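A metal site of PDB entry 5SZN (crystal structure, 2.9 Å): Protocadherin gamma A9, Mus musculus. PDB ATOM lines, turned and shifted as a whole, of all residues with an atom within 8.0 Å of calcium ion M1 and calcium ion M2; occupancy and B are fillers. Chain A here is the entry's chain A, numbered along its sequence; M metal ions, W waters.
The side-chain carboxylate (OE2) of Glu 330 binds calcium ion M1, 2.3 Å away.
OD1 of Asp 419 binds calcium ion M1, 2.4 Å away.
Calcium ion M1 is bound by the side-chain carboxylate (OE1) of Glu 330 (2.5 Å).
Calcium ion M1 is bound by OD2 of Asp 419, 2.6 Å away.
Water W1 binds calcium ion M1 (2.7 Å).
Calcium ion M1 is bound by OE1 of Glu 385 (2.8 Å).
Calcium ion M1 has six donor atoms within binding distance.
Arg 384 touches calcium ion M2.
Within 4 Å of calcium ion M2: Glu 330, Arg 384, Glu 385, Asp 416, Ile 417, Asp 419 and Asp 452.
The side-chain carboxylate (OE2) of Glu 330 lies close to the backbone NH (N) of Arg 384.
N of Asn 420 is in hydrogen-bond range of OD2 of Asp 452 (3.4 Å).
OD2 of Asp 452 lies close to OD1 of Asn 418 (2.6 Å).
The backbone NH of Asp 452 lies close to the side-chain carboxylate of Asp 450, 3.0 Å away.
The guanidinium group (NH1) of Arg 384 lies within salt-bridge range of the side-chain carboxylate (OD2) of Asp 416 (3.8 Å).
OD2 of Asp 416 sits at hydrogen-bond distance from N of Asp 453 (2.9 Å).
NH1 of Arg 384 lies close to OE2 of Glu 385.
The guanidinium group (NH2) of Arg 384 is in salt-bridge range of the side-chain carboxylate (OD2) of Asp 453 (3.8 Å).
Residues that only touch calcium ion M1: Asp 383 and Asn 420.
Calcium ion M2 is bound by OD1 of Asp 452 (2.4 Å).
Calcium ion M2 is bound by OD1 of Asp 416, 2.5 Å away.
OE2 of Glu 385 is bound to calcium ion M2 (2.7 Å).
Calcium ion M2 has three donor atoms within binding distance.
Slightly farther from calcium ion M2 lies O of Ile 417 (3.0 Å).
Slightly farther from calcium ion M2 lies the side-chain carboxylate (OE1) of Glu 330 (3.1 Å).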
ATOM      1  N   GLU A 330     -16.377 -17.664   0.817  1.00  0.00           N
ATOM      2  CA  GLU A 330     -16.915 -16.709  -0.139  1.00  0.00           C
ATOM      3  C   GLU A 330     -17.583 -15.525   0.564  1.00  0.00           C
ATOM      4  O   GLU A 330     -17.635 -14.426   0.007  1.00  0.00           O
ATOM      5  CB  GLU A 330     -17.902 -17.414  -1.075  1.00  0.00           C
ATOM      6  CG  GLU A 330     -18.441 -16.553  -2.199  1.00  0.00           C
ATOM      7  CD  GLU A 330     -19.623 -17.208  -2.889  1.00  0.00           C
ATOM      8  OE1 GLU A 330     -20.054 -18.284  -2.436  1.00  0.00           O
ATOM      9  OE2 GLU A 330     -20.115 -16.641  -3.891  1.00  0.00           O
ATOM     10  N   ASP A 331     -18.079 -15.735   1.778  1.00  0.00           N
ATOM     11  CA  ASP A 331     -18.741 -14.692   2.550  1.00  0.00           C
ATOM     12  C   ASP A 331     -17.773 -13.728   3.221  1.00  0.00           C
ATOM     13  O   ASP A 331     -18.201 -12.910   4.047  1.00  0.00           O
ATOM     14  CB  ASP A 331     -19.647 -15.326   3.616  1.00  0.00           C
ATOM     15  CG  ASP A 331     -18.898 -16.286   4.537  1.00  0.00           C
ATOM     16  OD1 ASP A 331     -17.723 -16.014   4.876  1.00  0.00           O
ATOM     17  OD2 ASP A 331     -19.495 -17.312   4.938  1.00  0.00           O
ATOM     18  N   ILE A 381     -16.186  -8.392  -2.022  1.00  0.00           N
ATOM     19  CA  ILE A 381     -16.738  -9.699  -1.695  1.00  0.00           C
ATOM     20  C   ILE A 381     -16.514 -10.639  -2.868  1.00  0.00           C
ATOM     21  O   ILE A 381     -16.708 -10.263  -4.035  1.00  0.00           O
ATOM     22  CB  ILE A 381     -18.231  -9.595  -1.327  1.00  0.00           C
ATOM     23  CG1 ILE A 381     -18.397  -8.989   0.072  1.00  0.00           C
ATOM     24  CG2 ILE A 381     -18.904 -10.953  -1.369  1.00  0.00           C
ATOM     25  CD1 ILE A 381     -18.640  -7.513   0.069  1.00  0.00           C
ATOM     26  N   LEU A 382     -16.117 -11.871  -2.569  1.00  0.00           N
ATOM     27  CA  LEU A 382     -15.870 -12.879  -3.586  1.00  0.00           C
ATOM     28  C   LEU A 382     -17.156 -13.592  -3.974  1.00  0.00           C
ATOM     29  O   LEU A 382     -18.175 -13.523  -3.281  1.00  0.00           O
ATOM     30  CB  LEU A 382     -14.830 -13.897  -3.101  1.00  0.00           C
ATOM     31  CG  LEU A 382     -13.380 -13.428  -2.932  1.00  0.00           C
ATOM     32  CD1 LEU A 382     -12.944 -12.614  -4.138  1.00  0.00           C
ATOM     33  CD2 LEU A 382     -13.179 -12.631  -1.646  1.00  0.00           C
ATOM     34  N   ASP A 383     -17.109 -14.285  -5.111  1.00  0.00           N
ATOM     35  CA  ASP A 383     -18.277 -14.985  -5.632  1.00  0.00           C
ATOM     36  C   ASP A 383     -17.774 -16.089  -6.565  1.00  0.00           C
ATOM     37  O   ASP A 383     -17.451 -15.817  -7.724  1.00  0.00           O
ATOM     38  CB  ASP A 383     -19.217 -14.031  -6.362  1.00  0.00           C
ATOM     39  CG  ASP A 383     -20.372 -14.735  -7.033  1.00  0.00           C
ATOM     40  OD1 ASP A 383     -20.937 -15.668  -6.419  1.00  0.00           O
ATOM     41  OD2 ASP A 383     -20.716 -14.369  -8.168  1.00  0.00           O
ATOM     42  N   ARG A 384     -17.707 -17.315  -6.060  1.00  0.00           N
ATOM     43  CA  ARG A 384     -17.075 -18.399  -6.793  1.00  0.00           C
ATOM     44  C   ARG A 384     -17.907 -18.891  -7.978  1.00  0.00           C
ATOM     45  O   ARG A 384     -17.404 -19.720  -8.754  1.00  0.00           O
ATOM     46  CB  ARG A 384     -16.783 -19.576  -5.863  1.00  0.00           C
ATOM     47  CG  ARG A 384     -18.005 -20.187  -5.222  1.00  0.00           C
ATOM     48  CD  ARG A 384     -17.625 -21.423  -4.440  1.00  0.00           C
ATOM     49  NE  ARG A 384     -17.071 -22.466  -5.301  1.00  0.00           N
ATOM     50  CZ  ARG A 384     -17.796 -23.405  -5.906  1.00  0.00           C
ATOM     51  NH1 ARG A 384     -19.116 -23.427  -5.751  1.00  0.00           N
ATOM     52  NH2 ARG A 384     -17.209 -24.319  -6.662  1.00  0.00           N
ATOM     53  N   GLU A 385     -19.145 -18.432  -8.128  1.00  0.00           N
ATOM     54  CA  GLU A 385     -19.917 -18.770  -9.319  1.00  0.00           C
ATOM     55  C   GLU A 385     -19.522 -17.917 -10.520  1.00  0.00           C
ATOM     56  O   GLU A 385     -19.937 -18.236 -11.640  1.00  0.00           O
ATOM     57  CB  GLU A 385     -21.409 -18.644  -9.044  1.00  0.00           C
ATOM     58  CG  GLU A 385     -22.001 -19.829  -8.303  1.00  0.00           C
ATOM     59  CD  GLU A 385     -21.586 -19.889  -6.844  1.00  0.00           C
ATOM     60  OE1 GLU A 385     -21.470 -18.827  -6.212  1.00  0.00           O
ATOM     61  OE2 GLU A 385     -21.367 -21.016  -6.328  1.00  0.00           O
ATOM     62  N   LYS A 386     -18.767 -16.844 -10.309  1.00  0.00           N
ATOM     63  CA  LYS A 386     -18.175 -16.071 -11.390  1.00  0.00           C
ATOM     64  C   LYS A 386     -16.673 -16.276 -11.531  1.00  0.00           C
ATOM     65  O   LYS A 386     -16.151 -16.156 -12.642  1.00  0.00           O
ATOM     66  CB  LYS A 386     -18.449 -14.572 -11.196  1.00  0.00           C
ATOM     67  N   ALA A 415     -13.446 -20.802  -1.213  1.00  0.00           N
ATOM     68  CA  ALA A 415     -14.269 -21.894  -0.731  1.00  0.00           C
ATOM     69  C   ALA A 415     -15.732 -21.648  -1.077  1.00  0.00           C
ATOM     70  O   ALA A 415     -16.123 -20.585  -1.573  1.00  0.00           O
ATOM     71  CB  ALA A 415     -14.105 -22.057   0.780  1.00  0.00           C
ATOM     72  N   ASP A 416     -16.563 -22.655  -0.806  1.00  0.00           N
ATOM     73  CA  ASP A 416     -17.969 -22.638  -1.188  1.00  0.00           C
ATOM     74  C   ASP A 416     -18.832 -22.406   0.050  1.00  0.00           C
ATOM     75  O   ASP A 416     -18.837 -23.229   0.971  1.00  0.00           O
ATOM     76  CB  ASP A 416     -18.383 -23.936  -1.879  1.00  0.00           C
ATOM     77  CG  ASP A 416     -19.808 -23.903  -2.393  1.00  0.00           C
ATOM     78  OD1 ASP A 416     -20.333 -22.797  -2.631  1.00  0.00           O
ATOM     79  OD2 ASP A 416     -20.418 -24.983  -2.553  1.00  0.00           O
ATOM     80  N   ILE A 417     -19.560 -21.301   0.054  1.00  0.00           N
ATOM     81  CA  ILE A 417     -20.588 -21.009   1.054  1.00  0.00           C
ATOM     82  C   ILE A 417     -21.936 -21.103   0.369  1.00  0.00           C
ATOM     83  O   ILE A 417     -22.132 -20.534  -0.716  1.00  0.00           O
ATOM     84  CB  ILE A 417     -20.373 -19.625   1.696  1.00  0.00           C
ATOM     85  CG1 ILE A 417     -19.051 -19.597   2.477  1.00  0.00           C
ATOM     86  CG2 ILE A 417     -21.533 -19.279   2.614  1.00  0.00           C
ATOM     87  CD1 ILE A 417     -18.973 -20.640   3.569  1.00  0.00           C
ATOM     88  N   ASN A 418     -22.871 -21.822   0.990  1.00  0.00           N
ATOM     89  CA  ASN A 418     -24.152 -22.151   0.375  1.00  0.00           C
ATOM     90  C   ASN A 418     -25.071 -20.930   0.427  1.00  0.00           C
ATOM     91  O   ASN A 418     -25.690 -20.643   1.452  1.00  0.00           O
ATOM     92  CB  ASN A 418     -24.784 -23.344   1.081  1.00  0.00           C
ATOM     93  CG  ASN A 418     -26.019 -23.847   0.365  1.00  0.00           C
ATOM     94  OD1 ASN A 418     -26.295 -23.475  -0.778  1.00  0.00           O
ATOM     95  ND2 ASN A 418     -26.780 -24.718   1.030  1.00  0.00           N
ATOM     96  N   ASP A 419     -25.167 -20.218  -0.693  1.00  0.00           N
ATOM     97  CA  ASP A 419     -26.090 -19.096  -0.832  1.00  0.00           C
ATOM     98  C   ASP A 419     -26.915 -19.180  -2.102  1.00  0.00           C
ATOM     99  O   ASP A 419     -27.591 -18.206  -2.452  1.00  0.00           O
ATOM    100  CB  ASP A 419     -25.322 -17.768  -0.787  1.00  0.00           C
ATOM    101  CG  ASP A 419     -24.242 -17.677  -1.852  1.00  0.00           C
ATOM    102  OD1 ASP A 419     -23.686 -18.725  -2.214  1.00  0.00           O
ATOM    103  OD2 ASP A 419     -23.960 -16.555  -2.317  1.00  0.00           O
ATOM    104  N   ASN A 420     -26.902 -20.316  -2.802  1.00  0.00           N
ATOM    105  CA  ASN A 420     -27.654 -20.495  -4.042  1.00  0.00           C
ATOM    106  C   ASN A 420     -28.583 -21.684  -3.907  1.00  0.00           C
ATOM    107  O   ASN A 420     -28.111 -22.811  -3.672  1.00  0.00           O
ATOM    108  CB  ASN A 420     -26.704 -20.678  -5.222  1.00  0.00           C
ATOM    109  CG  ASN A 420     -25.850 -19.452  -5.475  1.00  0.00           C
ATOM    110  OD1 ASN A 420     -26.252 -18.333  -5.181  1.00  0.00           O
ATOM    111  ND2 ASN A 420     -24.661 -19.671  -6.033  1.00  0.00           N
ATOM    112  N   ASP A 450     -28.109 -27.024  -9.015  1.00  0.00           N
ATOM    113  CA  ASP A 450     -27.685 -26.102  -7.965  1.00  0.00           C
ATOM    114  C   ASP A 450     -26.331 -25.509  -8.343  1.00  0.00           C
ATOM    115  O   ASP A 450     -25.402 -26.257  -8.679  1.00  0.00           O
ATOM    116  CB  ASP A 450     -27.613 -26.813  -6.615  1.00  0.00           C
ATOM    117  CG  ASP A 450     -27.519 -25.844  -5.443  1.00  0.00           C
ATOM    118  OD1 ASP A 450     -26.706 -24.902  -5.498  1.00  0.00           O
ATOM    119  OD2 ASP A 450     -28.256 -26.044  -4.449  1.00  0.00           O
ATOM    120  N   PRO A 451     -26.175 -24.180  -8.314  1.00  0.00           N
ATOM    121  CA  PRO A 451     -24.903 -23.589  -8.723  1.00  0.00           C
ATOM    122  C   PRO A 451     -23.733 -23.916  -7.813  1.00  0.00           C
ATOM    123  O   PRO A 451     -22.588 -23.914  -8.275  1.00  0.00           O
ATOM    124  CB  PRO A 451     -25.200 -22.081  -8.718  1.00  0.00           C
ATOM    125  CG  PRO A 451     -26.679 -21.982  -8.835  1.00  0.00           C
ATOM    126  CD  PRO A 451     -27.226 -23.163  -8.096  1.00  0.00           C
ATOM    127  N   ASP A 452     -23.986 -24.201  -6.537  1.00  0.00           N
ATOM    128  CA  ASP A 452     -22.899 -24.456  -5.586  1.00  0.00           C
ATOM    129  C   ASP A 452     -22.208 -25.780  -5.925  1.00  0.00           C
ATOM    130  O   ASP A 452     -22.479 -26.419  -6.942  1.00  0.00           O
ATOM    131  CB  ASP A 452     -23.444 -24.451  -4.154  1.00  0.00           C
ATOM    132  CG  ASP A 452     -23.859 -23.075  -3.694  1.00  0.00           C
ATOM    133  OD1 ASP A 452     -23.321 -22.081  -4.232  1.00  0.00           O
ATOM    134  OD2 ASP A 452     -24.713 -22.979  -2.799  1.00  0.00           O
ATOM    135  N   ASP A 453     -21.293 -26.198  -5.058  1.00  0.00           N
ATOM    136  CA  ASP A 453     -20.484 -27.379  -5.316  1.00  0.00           C
ATOM    137  C   ASP A 453     -20.633 -28.381  -4.170  1.00  0.00           C
ATOM    138  O   ASP A 453     -20.893 -27.999  -3.024  1.00  0.00           O
ATOM    139  CB  ASP A 453     -19.006 -27.019  -5.496  1.00  0.00           C
ATOM    140  CG  ASP A 453     -18.185 -28.176  -6.027  1.00  0.00           C
ATOM    141  OD1 ASP A 453     -18.784 -29.184  -6.475  1.00  0.00           O
ATOM    142  OD2 ASP A 453     -16.940 -28.081  -6.020  1.00  0.00           O
ATOM    143  N   ASN A 456     -23.643 -28.856  -1.155  1.00  0.00           N
ATOM    144  CA  ASN A 456     -24.548 -27.731  -1.388  1.00  0.00           C
ATOM    145  C   ASN A 456     -25.093 -27.703  -2.805  1.00  0.00           C
ATOM    146  O   ASN A 456     -25.732 -26.721  -3.208  1.00  0.00           O
ATOM    147  CB  ASN A 456     -23.836 -26.421  -1.065  1.00  0.00           C
ATOM    148  CG  ASN A 456     -23.330 -26.381   0.369  1.00  0.00           C
ATOM    149  OD1 ASN A 456     -23.838 -27.075   1.242  1.00  0.00           O
ATOM    150  ND2 ASN A 456     -22.311 -25.551   0.607  1.00  0.00           N
HETATM  151 CA    CA M   1     -22.116 -17.681  -3.740  1.00  0.00          CA
HETATM  152 CA    CA M   2     -21.388 -20.782  -3.589  1.00  0.00          CA
HETATM  153 CA    CA M   3     -27.067 -24.821  -2.664  1.00  0.00          CA
HETATM  154  O   HOH W   1     -22.869 -16.741  -6.112  1.00  0.00           O
